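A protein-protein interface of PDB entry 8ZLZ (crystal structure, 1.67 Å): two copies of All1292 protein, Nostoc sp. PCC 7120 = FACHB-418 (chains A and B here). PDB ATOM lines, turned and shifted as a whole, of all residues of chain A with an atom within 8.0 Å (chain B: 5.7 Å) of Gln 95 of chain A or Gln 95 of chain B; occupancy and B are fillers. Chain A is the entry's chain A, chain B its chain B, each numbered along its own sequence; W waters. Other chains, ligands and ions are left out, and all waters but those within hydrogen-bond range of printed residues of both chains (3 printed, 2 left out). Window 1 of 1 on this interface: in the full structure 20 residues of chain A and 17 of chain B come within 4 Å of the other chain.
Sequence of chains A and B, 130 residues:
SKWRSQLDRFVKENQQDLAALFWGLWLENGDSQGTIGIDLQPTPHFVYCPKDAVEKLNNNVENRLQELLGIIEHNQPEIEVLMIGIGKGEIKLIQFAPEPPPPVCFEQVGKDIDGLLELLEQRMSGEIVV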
ATOM      1  N   ASP A   8      10.658 -12.966 -20.683  1.00  0.00           N
ATOM      2  CA  ASP A   8      11.413 -12.410 -19.573  1.00  0.00           C
ATOM      3  C   ASP A   8      12.720 -13.164 -19.345  1.00  0.00           C
ATOM      4  O   ASP A   8      13.760 -12.544 -19.100  1.00  0.00           O
ATOM      5  CB  ASP A   8      10.573 -12.408 -18.302  1.00  0.00           C
ATOM      6  CG  ASP A   8      11.162 -11.492 -17.246  1.00  0.00           C
ATOM      7  OD1 ASP A   8      11.146 -10.243 -17.423  1.00  0.00           O
ATOM      8  OD2 ASP A   8      11.689 -12.044 -16.274  1.00  0.00           O
ATOM      9  N   VAL A  11      15.135 -12.183 -22.101  1.00  0.00           N
ATOM     10  CA  VAL A  11      15.720 -10.868 -21.854  1.00  0.00           C
ATOM     11  C   VAL A  11      16.835 -10.948 -20.811  1.00  0.00           C
ATOM     12  O   VAL A  11      17.915 -10.375 -20.999  1.00  0.00           O
ATOM     13  CB  VAL A  11      14.625  -9.863 -21.443  1.00  0.00           C
ATOM     14  CG1 VAL A  11      15.267  -8.575 -20.919  1.00  0.00           C
ATOM     15  CG2 VAL A  11      13.755  -9.541 -22.654  1.00  0.00           C
ATOM     16  N   GLN A  15      20.832  -9.580 -22.100  1.00  0.00           N
ATOM     17  CA  GLN A  15      20.821  -8.136 -21.847  1.00  0.00           C
ATOM     18  C   GLN A  15      21.909  -7.406 -22.634  1.00  0.00           C
ATOM     19  O   GLN A  15      21.678  -6.294 -23.127  1.00  0.00           O
ATOM     20  CB  GLN A  15      20.978  -7.864 -20.353  1.00  0.00           C
ATOM     21  CG  GLN A  15      19.729  -8.146 -19.555  1.00  0.00           C
ATOM     22  CD  GLN A  15      19.826  -7.601 -18.148  1.00  0.00           C
ATOM     23  OE1 GLN A  15      20.821  -6.978 -17.777  1.00  0.00           O
ATOM     24  NE2 GLN A  15      18.792  -7.830 -17.355  1.00  0.00           N
ATOM     25  N   GLY A  70       4.529   7.602 -19.436  1.00  0.00           N
ATOM     26  CA  GLY A  70       5.526   8.257 -18.609  1.00  0.00           C
ATOM     27  C   GLY A  70       6.779   7.417 -18.455  1.00  0.00           C
ATOM     28  O   GLY A  70       7.894   7.934 -18.533  1.00  0.00           O
ATOM     29  N   ILE A  71       6.611   6.107 -18.235  1.00  0.00           N
ATOM     30  CA  ILE A  71       7.777   5.225 -18.134  1.00  0.00           C
ATOM     31  C   ILE A  71       8.608   5.308 -19.405  1.00  0.00           C
ATOM     32  O   ILE A  71       9.840   5.421 -19.361  1.00  0.00           O
ATOM     33  CB  ILE A  71       7.332   3.779 -17.842  1.00  0.00           C
ATOM     34  CG1 ILE A  71       6.660   3.692 -16.464  1.00  0.00           C
ATOM     35  CG2 ILE A  71       8.550   2.818 -17.905  1.00  0.00           C
ATOM     36  CD1 ILE A  71       6.123   2.274 -16.120  1.00  0.00           C
ATOM     37  N   ILE A  72       7.940   5.290 -20.557  1.00  0.00           N
ATOM     38  CA  ILE A  72       8.643   5.348 -21.838  1.00  0.00           C
ATOM     39  C   ILE A  72       9.368   6.681 -21.994  1.00  0.00           C
ATOM     40  O   ILE A  72      10.532   6.724 -22.408  1.00  0.00           O
ATOM     41  CB  ILE A  72       7.642   5.098 -22.977  1.00  0.00           C
ATOM     42  CG1 ILE A  72       7.226   3.627 -22.968  1.00  0.00           C
ATOM     43  CG2 ILE A  72       8.231   5.521 -24.332  1.00  0.00           C
ATOM     44  CD1 ILE A  72       5.987   3.341 -23.828  1.00  0.00           C
ATOM     45  N   HIS A  74      10.413   8.681 -19.613  1.00  0.00           N
ATOM     46  CA  HIS A  74      11.414   8.906 -18.577  1.00  0.00           C
ATOM     47  C   HIS A  74      12.627   7.998 -18.688  1.00  0.00           C
ATOM     48  O   HIS A  74      13.678   8.336 -18.138  1.00  0.00           O
ATOM     49  CB  HIS A  74      10.787   8.752 -17.198  1.00  0.00           C
ATOM     50  CG  HIS A  74       9.795   9.825 -16.896  1.00  0.00           C
ATOM     51  ND1 HIS A  74       8.616   9.574 -16.239  1.00  0.00           N
ATOM     52  CD2 HIS A  74       9.782  11.142 -17.221  1.00  0.00           C
ATOM     53  CE1 HIS A  74       7.924  10.696 -16.137  1.00  0.00           C
ATOM     54  NE2 HIS A  74       8.612  11.667 -16.718  1.00  0.00           N
ATOM     55  N   ASN A  75      12.525   6.888 -19.412  1.00  0.00           N
ATOM     56  CA  ASN A  75      13.673   6.002 -19.594  1.00  0.00           C
ATOM     57  C   ASN A  75      14.841   6.774 -20.192  1.00  0.00           C
ATOM     58  O   ASN A  75      14.661   7.522 -21.161  1.00  0.00           O
ATOM     59  CB  ASN A  75      13.280   4.840 -20.515  1.00  0.00           C
ATOM     60  CG  ASN A  75      14.353   3.781 -20.599  1.00  0.00           C
ATOM     61  OD1 ASN A  75      14.493   2.961 -19.688  1.00  0.00           O
ATOM     62  ND2 ASN A  75      15.163   3.826 -21.667  1.00  0.00           N
ATOM     63  N   GLN A  76      16.030   6.631 -19.583  1.00  0.00           N
ATOM     64  CA  GLN A  76      17.212   7.347 -20.049  1.00  0.00           C
ATOM     65  C   GLN A  76      18.076   6.387 -20.850  1.00  0.00           C
ATOM     66  O   GLN A  76      18.706   5.493 -20.263  1.00  0.00           O
ATOM     67  CB  GLN A  76      17.998   7.940 -18.881  1.00  0.00           C
ATOM     68  CG  GLN A  76      17.177   8.910 -17.970  1.00  0.00           C
ATOM     69  CD  GLN A  76      16.741  10.215 -18.674  1.00  0.00           C
ATOM     70  OE1 GLN A  76      16.770  10.320 -19.912  1.00  0.00           O
ATOM     71  NE2 GLN A  76      16.366  11.231 -17.874  1.00  0.00           N
ATOM     72  N   ILE A  79      21.583   4.978 -20.144  1.00  0.00           N
ATOM     73  CA  ILE A  79      21.707   4.180 -18.931  1.00  0.00           C
ATOM     74  C   ILE A  79      20.917   2.882 -19.030  1.00  0.00           C
ATOM     75  O   ILE A  79      21.332   1.859 -18.480  1.00  0.00           O
ATOM     76  CB  ILE A  79      21.243   4.976 -17.690  1.00  0.00           C
ATOM     77  CG1 ILE A  79      21.887   6.354 -17.613  1.00  0.00           C
ATOM     78  CG2 ILE A  79      21.583   4.211 -16.424  1.00  0.00           C
ATOM     79  CD1 ILE A  79      21.172   7.247 -16.621  1.00  0.00           C
ATOM     80  N   GLU A  80      19.749   2.917 -19.670  1.00  0.00           N
ATOM     81  CA  GLU A  80      18.766   1.861 -19.470  1.00  0.00           C
ATOM     82  C   GLU A  80      18.114   1.504 -20.787  1.00  0.00           C
ATOM     83  O   GLU A  80      17.770   2.395 -21.570  1.00  0.00           O
ATOM     84  CB  GLU A  80      17.600   2.300 -18.610  1.00  0.00           C
ATOM     85  CG  GLU A  80      17.807   3.403 -17.687  1.00  0.00           C
ATOM     86  CD  GLU A  80      16.521   3.668 -16.982  1.00  0.00           C
ATOM     87  OE1 GLU A  80      16.090   2.676 -16.354  1.00  0.00           O
ATOM     88  OE2 GLU A  80      15.971   4.806 -17.062  1.00  0.00           O
ATOM     89  N   VAL A  81      17.821   0.213 -20.965  1.00  0.00           N
ATOM     90  CA  VAL A  81      17.082  -0.281 -22.127  1.00  0.00           C
ATOM     91  C   VAL A  81      15.595  -0.328 -21.813  1.00  0.00           C
ATOM     92  O   VAL A  81      15.200  -0.760 -20.728  1.00  0.00           O
ATOM     93  CB  VAL A  81      17.595  -1.681 -22.514  1.00  0.00           C
ATOM     94  CG1 VAL A  81      16.702  -2.346 -23.574  1.00  0.00           C
ATOM     95  CG2 VAL A  81      19.059  -1.579 -23.001  1.00  0.00           C
ATOM     96  N   LEU A  82      14.766   0.054 -22.794  1.00  0.00           N
ATOM     97  CA  LEU A  82      13.322  -0.146 -22.723  1.00  0.00           C
ATOM     98  C   LEU A  82      12.837  -0.680 -24.059  1.00  0.00           C
ATOM     99  O   LEU A  82      13.161  -0.100 -25.108  1.00  0.00           O
ATOM    100  CB  LEU A  82      12.587   1.165 -22.377  1.00  0.00           C
ATOM    101  CG  LEU A  82      11.086   0.990 -22.134  1.00  0.00           C
ATOM    102  CD1 LEU A  82      10.609   2.011 -21.111  1.00  0.00           C
ATOM    103  CD2 LEU A  82      10.282   1.155 -23.445  1.00  0.00           C
ATOM    104  N   MET A  83      12.096  -1.797 -24.015  1.00  0.00           N
ATOM    105  CA  MET A  83      11.282  -2.210 -25.149  1.00  0.00           C
ATOM    106  C   MET A  83       9.964  -2.747 -24.642  1.00  0.00           C
ATOM    107  O   MET A  83       9.726  -2.808 -23.443  1.00  0.00           O
ATOM    108  CB  MET A  83      11.947  -3.214 -26.123  1.00  0.00           C
ATOM    109  CG  MET A  83      13.452  -3.097 -26.392  1.00  0.00           C
ATOM    110  SD  MET A  83      14.262  -4.620 -26.911  1.00  0.00           S
ATOM    111  CE  MET A  83      15.894  -3.964 -27.337  1.00  0.00           C
ATOM    112  N   ILE A  84       9.073  -3.102 -25.563  1.00  0.00           N
ATOM    113  CA  ILE A  84       7.832  -3.757 -25.175  1.00  0.00           C
ATOM    114  C   ILE A  84       7.696  -5.053 -25.951  1.00  0.00           C
ATOM    115  O   ILE A  84       8.000  -5.114 -27.149  1.00  0.00           O
ATOM    116  CB  ILE A  84       6.586  -2.860 -25.372  1.00  0.00           C
ATOM    117  CG1 ILE A  84       6.433  -2.410 -26.827  1.00  0.00           C
ATOM    118  CG2 ILE A  84       6.621  -1.676 -24.396  1.00  0.00           C
ATOM    119  CD1 ILE A  84       5.107  -1.695 -27.090  1.00  0.00           C
ATOM    120  N   LYS A  92       4.041  -6.584 -22.570  1.00  0.00           N
ATOM    121  CA  LYS A  92       4.963  -6.886 -21.473  1.00  0.00           C
ATOM    122  C   LYS A  92       6.098  -5.874 -21.542  1.00  0.00           C
ATOM    123  O   LYS A  92       6.766  -5.768 -22.572  1.00  0.00           O
ATOM    124  CB  LYS A  92       5.515  -8.309 -21.576  1.00  0.00           C
ATOM    125  CG  LYS A  92       6.457  -8.713 -20.416  1.00  0.00           C
ATOM    126  CD  LYS A  92       7.911  -8.750 -20.889  1.00  0.00           C
ATOM    127  CE  LYS A  92       8.806  -9.488 -19.898  1.00  0.00           C
ATOM    128  NZ  LYS A  92       9.285  -8.624 -18.802  1.00  0.00           N
ATOM    129  N   LEU A  93       6.304  -5.116 -20.467  1.00  0.00           N
ATOM    130  CA  LEU A  93       7.367  -4.119 -20.480  1.00  0.00           C
ATOM    131  C   LEU A  93       8.715  -4.798 -20.304  1.00  0.00           C
ATOM    132  O   LEU A  93       8.879  -5.655 -19.428  1.00  0.00           O
ATOM    133  CB  LEU A  93       7.168  -3.078 -19.378  1.00  0.00           C
ATOM    134  CG  LEU A  93       8.261  -1.999 -19.314  1.00  0.00           C
ATOM    135  CD1 LEU A  93       8.262  -1.081 -20.571  1.00  0.00           C
ATOM    136  CD2 LEU A  93       8.090  -1.160 -18.058  1.00  0.00           C
ATOM    137  N   ILE A  94       9.674  -4.403 -21.134  1.00  0.00           N
ATOM    138  CA  ILE A  94      11.065  -4.833 -21.019  1.00  0.00           C
ATOM    139  C   ILE A  94      11.868  -3.621 -20.572  1.00  0.00           C
ATOM    140  O   ILE A  94      11.930  -2.611 -21.286  1.00  0.00           O
ATOM    141  CB  ILE A  94      11.600  -5.385 -22.349  1.00  0.00           C
ATOM    142  CG1 ILE A  94      10.810  -6.648 -22.753  1.00  0.00           C
ATOM    143  CG2 ILE A  94      13.112  -5.625 -22.256  1.00  0.00           C
ATOM    144  CD1 ILE A  94      11.047  -7.098 -24.198  1.00  0.00           C
ATOM    145  N   GLN A  95      12.467  -3.700 -19.391  1.00  0.00           N
ATOM    146  CA  GLN A  95      13.300  -2.591 -18.935  1.00  0.00           C
ATOM    147  C   GLN A  95      14.409  -3.111 -18.048  1.00  0.00           C
ATOM    148  O   GLN A  95      14.135  -3.892 -17.132  1.00  0.00           O
ATOM    149  CB  GLN A  95      12.483  -1.535 -18.158  1.00  0.00           C
ATOM    150  CG  GLN A  95      13.195  -0.197 -18.136  1.00  0.00           C
ATOM    151  CD  GLN A  95      12.492   0.876 -17.319  1.00  0.00           C
ATOM    152  OE1 GLN A  95      12.665   2.075 -17.590  1.00  0.00           O
ATOM    153  NE2 GLN A  95      11.733   0.470 -16.315  1.00  0.00           N
ATOM    154  N   PHE A  96      15.636  -2.659 -18.307  1.00  0.00           N
ATOM    155  CA  PHE A  96      16.762  -3.064 -17.472  1.00  0.00           C
ATOM    156  C   PHE A  96      17.918  -2.097 -17.695  1.00  0.00           C
ATOM    157  O   PHE A  96      18.086  -1.556 -18.788  1.00  0.00           O
ATOM    158  CB  PHE A  96      17.194  -4.508 -17.776  1.00  0.00           C
ATOM    159  CG  PHE A  96      17.578  -4.744 -19.212  1.00  0.00           C
ATOM    160  CD1 PHE A  96      16.622  -5.137 -20.146  1.00  0.00           C
ATOM    161  CD2 PHE A  96      18.900  -4.595 -19.627  1.00  0.00           C
ATOM    162  CE1 PHE A  96      16.957  -5.357 -21.482  1.00  0.00           C
ATOM    163  CE2 PHE A  96      19.264  -4.821 -20.975  1.00  0.00           C
ATOM    164  CZ  PHE A  96      18.288  -5.207 -21.905  1.00  0.00           C
ATOM    165  N   ALA A  97      18.699  -1.860 -16.627  1.00  0.00           N
ATOM    166  CA  ALA A  97      19.893  -1.030 -16.725  1.00  0.00           C
ATOM    167  C   ALA A  97      21.092  -1.962 -16.800  1.00  0.00           C
ATOM    168  O   ALA A  97      21.502  -2.519 -15.765  1.00  0.00           O
ATOM    169  CB  ALA A  97      20.013  -0.089 -15.521  1.00  0.00           C
ATOM    170  N   PRO A  98      21.665  -2.207 -17.976  1.00  0.00           N
ATOM    171  CA  PRO A  98      22.660  -3.279 -18.115  1.00  0.00           C
ATOM    172  C   PRO A  98      24.036  -2.841 -17.638  1.00  0.00           C
ATOM    173  O   PRO A  98      24.291  -1.671 -17.349  1.00  0.00           O
ATOM    174  CB  PRO A  98      22.696  -3.542 -19.620  1.00  0.00           C
ATOM    175  CG  PRO A  98      22.390  -2.167 -20.230  1.00  0.00           C
ATOM    176  CD  PRO A  98      21.407  -1.508 -19.246  1.00  0.00           C
ATOM    177  N   ILE B  71      14.883   9.770 -12.027  1.00  0.00           N
ATOM    178  CA  ILE B  71      14.513   8.358 -12.115  1.00  0.00           C
ATOM    179  C   ILE B  71      13.820   7.923 -10.831  1.00  0.00           C
ATOM    180  O   ILE B  71      12.809   7.203 -10.858  1.00  0.00           O
ATOM    181  CB  ILE B  71      15.756   7.503 -12.427  1.00  0.00           C
ATOM    182  CG1 ILE B  71      16.123   7.662 -13.904  1.00  0.00           C
ATOM    183  CG2 ILE B  71      15.509   6.025 -12.119  1.00  0.00           C
ATOM    184  CD1 ILE B  71      17.483   7.098 -14.288  1.00  0.00           C
ATOM    185  N   ASN B  75       9.708   6.689 -10.611  1.00  0.00           N
ATOM    186  CA  ASN B  75       9.619   5.233 -10.636  1.00  0.00           C
ATOM    187  C   ASN B  75       8.190   4.783 -10.382  1.00  0.00           C
ATOM    188  O   ASN B  75       7.477   5.373  -9.559  1.00  0.00           O
ATOM    189  CB  ASN B  75      10.547   4.608  -9.598  1.00  0.00           C
ATOM    190  CG  ASN B  75      10.693   3.096  -9.796  1.00  0.00           C
ATOM    191  OD1 ASN B  75      11.177   2.647 -10.833  1.00  0.00           O
ATOM    192  ND2 ASN B  75      10.239   2.309  -8.819  1.00  0.00           N
ATOM    193  N   GLN B  76       7.754   3.769 -11.133  1.00  0.00           N
ATOM    194  CA  GLN B  76       6.435   3.191 -10.932  1.00  0.00           C
ATOM    195  C   GLN B  76       6.605   1.869 -10.208  1.00  0.00           C
ATOM    196  O   GLN B  76       6.890   0.847 -10.855  1.00  0.00           O
ATOM    197  CB  GLN B  76       5.696   2.993 -12.261  1.00  0.00           C
ATOM    198  CG  GLN B  76       5.515   4.271 -13.044  1.00  0.00           C
ATOM    199  CD  GLN B  76       4.528   5.171 -12.334  1.00  0.00           C
ATOM    200  OE1 GLN B  76       3.610   4.685 -11.662  1.00  0.00           O
ATOM    201  NE2 GLN B  76       4.760   6.477 -12.395  1.00  0.00           N
ATOM    202  N   GLU B  80       8.216  -1.371 -11.865  1.00  0.00           N
ATOM    203  CA  GLU B  80       9.670  -1.215 -11.899  1.00  0.00           C
ATOM    204  C   GLU B  80      10.267  -1.365 -10.512  1.00  0.00           C
ATOM    205  O   GLU B  80       9.907  -0.628  -9.588  1.00  0.00           O
ATOM    206  CB  GLU B  80      10.075   0.156 -12.447  1.00  0.00           C
ATOM    207  CG  GLU B  80       9.493   0.493 -13.809  1.00  0.00           C
ATOM    208  CD  GLU B  80       9.728   1.938 -14.188  1.00  0.00           C
ATOM    209  OE1 GLU B  80       9.045   2.821 -13.633  1.00  0.00           O
ATOM    210  OE2 GLU B  80      10.608   2.199 -15.046  1.00  0.00           O
ATOM    211  N   VAL B  81      11.215  -2.282 -10.384  1.00  0.00           N
ATOM    212  CA  VAL B  81      12.087  -2.328  -9.217  1.00  0.00           C
ATOM    213  C   VAL B  81      13.174  -1.280  -9.393  1.00  0.00           C
ATOM    214  O   VAL B  81      13.791  -1.191 -10.462  1.00  0.00           O
ATOM    215  CB  VAL B  81      12.714  -3.724  -9.071  1.00  0.00           C
ATOM    216  CG1 VAL B  81      13.714  -3.735  -7.913  1.00  0.00           C
ATOM    217  CG2 VAL B  81      11.647  -4.783  -8.888  1.00  0.00           C
ATOM    218  N   LEU B  82      13.411  -0.482  -8.355  1.00  0.00           N
ATOM    219  CA  LEU B  82      14.455   0.540  -8.368  1.00  0.00           C
ATOM    220  C   LEU B  82      15.331   0.391  -7.132  1.00  0.00           C
ATOM    221  O   LEU B  82      14.817   0.364  -6.010  1.00  0.00           O
ATOM    222  CB  LEU B  82      13.844   1.955  -8.399  1.00  0.00           C
ATOM    223  CG  LEU B  82      14.831   3.114  -8.276  1.00  0.00           C
ATOM    224  CD1 LEU B  82      15.819   3.153  -9.411  1.00  0.00           C
ATOM    225  CD2 LEU B  82      14.040   4.435  -8.206  1.00  0.00           C
ATOM    226  N   MET B  83      16.650   0.338  -7.328  1.00  0.00           N
ATOM    227  CA  MET B  83      17.612   0.222  -6.233  1.00  0.00           C
ATOM    228  C   MET B  83      18.880   0.973  -6.618  1.00  0.00           C
ATOM    229  O   MET B  83      19.200   1.078  -7.800  1.00  0.00           O
ATOM    230  CB  MET B  83      17.894  -1.257  -5.999  1.00  0.00           C
ATOM    231  CG  MET B  83      16.780  -1.979  -5.203  1.00  0.00           C
ATOM    232  SD  MET B  83      17.314  -3.620  -4.680  1.00  0.00           S
ATOM    233  CE  MET B  83      15.711  -4.367  -4.296  1.00  0.00           C
ATOM    234  N   LEU B  93      22.914   2.326 -11.144  1.00  0.00           N
ATOM    235  CA  LEU B  93      21.462   2.191 -11.205  1.00  0.00           C
ATOM    236  C   LEU B  93      21.034   0.738 -11.360  1.00  0.00           C
ATOM    237  O   LEU B  93      21.506   0.027 -12.250  1.00  0.00           O
ATOM    238  CB  LEU B  93      20.900   2.988 -12.381  1.00  0.00           C
ATOM    239  CG  LEU B  93      19.368   2.891 -12.554  1.00  0.00           C
ATOM    240  CD1 LEU B  93      18.665   3.520 -11.355  1.00  0.00           C
ATOM    241  CD2 LEU B  93      18.879   3.562 -13.857  1.00  0.00           C
ATOM    242  N   ILE B  94      20.102   0.318 -10.519  1.00  0.00           N
ATOM    243  CA  ILE B  94      19.396  -0.943 -10.682  1.00  0.00           C
ATOM    244  C   ILE B  94      17.948  -0.584 -10.969  1.00  0.00           C
ATOM    245  O   ILE B  94      17.249  -0.066 -10.089  1.00  0.00           O
ATOM    246  CB  ILE B  94      19.511  -1.834  -9.430  1.00  0.00           C
ATOM    247  CG1 ILE B  94      20.983  -2.156  -9.138  1.00  0.00           C
ATOM    248  CG2 ILE B  94      18.671  -3.104  -9.606  1.00  0.00           C
ATOM    249  CD1 ILE B  94      21.237  -2.620  -7.682  1.00  0.00           C
ATOM    250  N   GLN B  95      17.495  -0.837 -12.198  1.00  0.00           N
ATOM    251  CA  GLN B  95      16.095  -0.589 -12.535  1.00  0.00           C
ATOM    252  C   GLN B  95      15.658  -1.638 -13.544  1.00  0.00           C
ATOM    253  O   GLN B  95      16.240  -1.743 -14.624  1.00  0.00           O
ATOM    254  CB  GLN B  95      15.868   0.831 -13.080  1.00  0.00           C
ATOM    255  CG  GLN B  95      14.356   1.192 -13.124  1.00  0.00           C
ATOM    256  CD  GLN B  95      14.059   2.656 -13.456  1.00  0.00           C
ATOM    257  OE1 GLN B  95      14.711   3.256 -14.307  1.00  0.00           O
ATOM    258  NE2 GLN B  95      13.055   3.228 -12.795  1.00  0.00           N
ATOM    259  N   PHE B  96      14.659  -2.435 -13.192  1.00  0.00           N
ATOM    260  CA  PHE B  96      14.213  -3.465 -14.113  1.00  0.00           C
ATOM    261  C   PHE B  96      12.729  -3.728 -13.896  1.00  0.00           C
ATOM    262  O   PHE B  96      12.194  -3.479 -12.809  1.00  0.00           O
ATOM    263  CB  PHE B  96      15.046  -4.762 -13.961  1.00  0.00           C
ATOM    264  CG  PHE B  96      14.960  -5.398 -12.600  1.00  0.00           C
ATOM    265  CD1 PHE B  96      15.852  -5.037 -11.590  1.00  0.00           C
ATOM    266  CD2 PHE B  96      13.997  -6.356 -12.327  1.00  0.00           C
ATOM    267  CE1 PHE B  96      15.764  -5.620 -10.321  1.00  0.00           C
ATOM    268  CE2 PHE B  96      13.905  -6.939 -11.066  1.00  0.00           C
ATOM    269  CZ  PHE B  96      14.782  -6.565 -10.062  1.00  0.00           C
ATOM    270  N   ALA B  97      12.065  -4.223 -14.947  1.00  0.00           N
ATOM    271  CA  ALA B  97      10.643  -4.567 -14.882  1.00  0.00           C
ATOM    272  C   ALA B  97      10.502  -6.080 -14.884  1.00  0.00           C
ATOM    273  O   ALA B  97      10.562  -6.710 -15.952  1.00  0.00           O
ATOM    274  CB  ALA B  97       9.881  -3.957 -16.065  1.00  0.00           C
HETATM  275  O   HOH W   1       5.218   6.977 -15.294  1.00  0.00           O
HETATM  276  O   HOH W   2      12.153  -6.274 -18.000  1.00  0.00           O
HETATM  277  O   HOH W   3      18.818  -3.384 -13.916  1.00  0.00           O
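Gln 95 of chain A touches just these residues of chain B: Glu 80 (2.4 Å), Gln 95 (3.9 Å), Phe 96 (3.1 Å) and Ala 97 (3.0 Å).
Of the printed residues of chain B, Ala 97 of chain A touches Leu 93 (3.6 Å) and Gln 95 (3.2 Å).
Leu 82 of chain B touches none of the printed residues of chain A.
Printed residues of chain A within 4 Å of Leu 93 of chain B: Ile 79, Glu 80 and Ala 97.
Printed residues of chain A within 4 Å of Gln 95 of chain B: Glu 80 (2.5 Å), Gln 95 (3.9 Å), Phe 96 (3.2 Å) and Ala 97 (3.2 Å).
The nearest residue of chain A that does not touch Gln 95 of chain B is Asn 75 of chain A (5.4 Å).
Water W2 bridges O of Ala 97 of chain B (2.6 Å) and N of Gln 95 of chain A (2.9 Å).
Water W1 lies within hydrogen-bond range of the side-chain amide nitrogen (NE2) of Gln 76 of chain B (3.0 Å) and the backbone NH (N) of Ile 71 of chain A (3.4 Å).
Water W3 bridges N of Ala 97 of chain A (3.1 Å) and O of Gln 95 of chain B (3.1 Å).
Ile 71 of chain A touches Gln 76 of chain B, but with the chains exchanged Gln 76 of chain A does not touch Ile 71 of chain B (4.1 Å).
Ile 71 of chain A touches Glu 80 of chain B, and with the chains exchanged Glu 80 of chain A touches Ile 71 of chain B.
Glu 80 of chain A touches Gln 95 of chain B, and with the chains exchanged Gln 95 of chain A touches Glu 80 of chain B.
Gln 95 of chain A touches Ala 97 of chain B, and with the chains exchanged Ala 97 of chain A touches Gln 95 of chain B.
12 positions are printed for both chains.
Of the 16 pairs that touch across the chains among the printed residues, 11 have their exchanged pair printed and touching as well.
The side-chain amide oxygen (OE1) of Gln 95 of chain B lies close to the side-chain carboxylate (OE1) of Glu 80 of chain A, 2.5 Å away.
The side-chain amide nitrogen of Gln 95 of chain A lies within hydrogen-bond range of the side-chain carboxylate of Glu 80 of chain B.
The backbone carbonyl oxygen (O) of Gln 95 of chain A sits at hydrogen-bond distance from the backbone NH (N) of Ala 97 of chain B.
The backbone carbonyl oxygen (O) of Gln 95 of chain B sits at hydrogen-bond distance from the backbone NH (N) of Ala 97 of chain A (3.2 Å).
OD1 of Asp 8 of chain A lies within salt-bridge range of NZ of Lys 92 of chain A.
The backbone carbonyl oxygen (O) of Phe 96 of chain A sits at hydrogen-bond distance from the backbone NH (N) of Val 81 of chain A, at 2.8 Å.
The side-chain amide oxygen of Asn 75 of chain B sits at hydrogen-bond distance from the side-chain amide nitrogen of Gln 95 of chain B, 2.8 Å away.
The backbone NH (N) of Gln 76 of chain B lies within hydrogen-bond range of the side-chain carboxylate (OE1) of Glu 80 of chain B.
NE2 of Gln 95 of chain B sits at hydrogen-bond distance from OE2 of Glu 80 of chain B.
N of Val 81 of chain B lies within hydrogen-bond range of O of Phe 96 of chain B (2.9 Å).
Hydrophobic or aromatic side chains of chain A that line the printed part of chain B: Ile 71, Ile 79, Leu 93 and Ala 97.
Of the 12 printed residues of chain B, 7 touch a printed residue of chain A.
Printed residues of chain B that touch a printed residue of chain A: Ile 71, Gln 76, Glu 80, Leu 93, Gln 95, Phe 96 and Ala 97.
Hydrophobic or aromatic side chains of chain B that line the printed part of chain A: Ile 71, Leu 93, Phe 96 and Ala 97.
Among the printed residues, no Asp or Glu carboxylate lies within 4 Å of a Lys or Arg side-chain nitrogen of the other chain.
Among the printed residues, pairs that only touch across the chains: Gln 95 of chain A with Phe 96 of chain B (3.1 Å), Phe 96 of chain A with Gln 95 of chain B (3.2 Å), Ile 71 of chain A with Glu 80 of chain B (3.6 Å), Ala 97 of chain A with Leu 93 of chain B (3.6 Å), Ile 71 of chain A with Gln 76 of chain B (3.7 Å), Lys 92 of chain A with Ala 97 of chain B (3.7 Å), Ile 79 of chain A with Leu 93 of chain B (3.8 Å), Glu 80 of chain A with Leu 93 of chain B (3.8 Å), Asp 8 of chain A with Ala 97 of chain B (3.9 Å), Leu 93 of chain A with Ala 97 of chain B (3.9 Å), Glu 80 of chain A with Ile 71 of chain B (3.9 Å) and Gln 95 of chain A with Gln 95 of chain B (3.9 Å).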
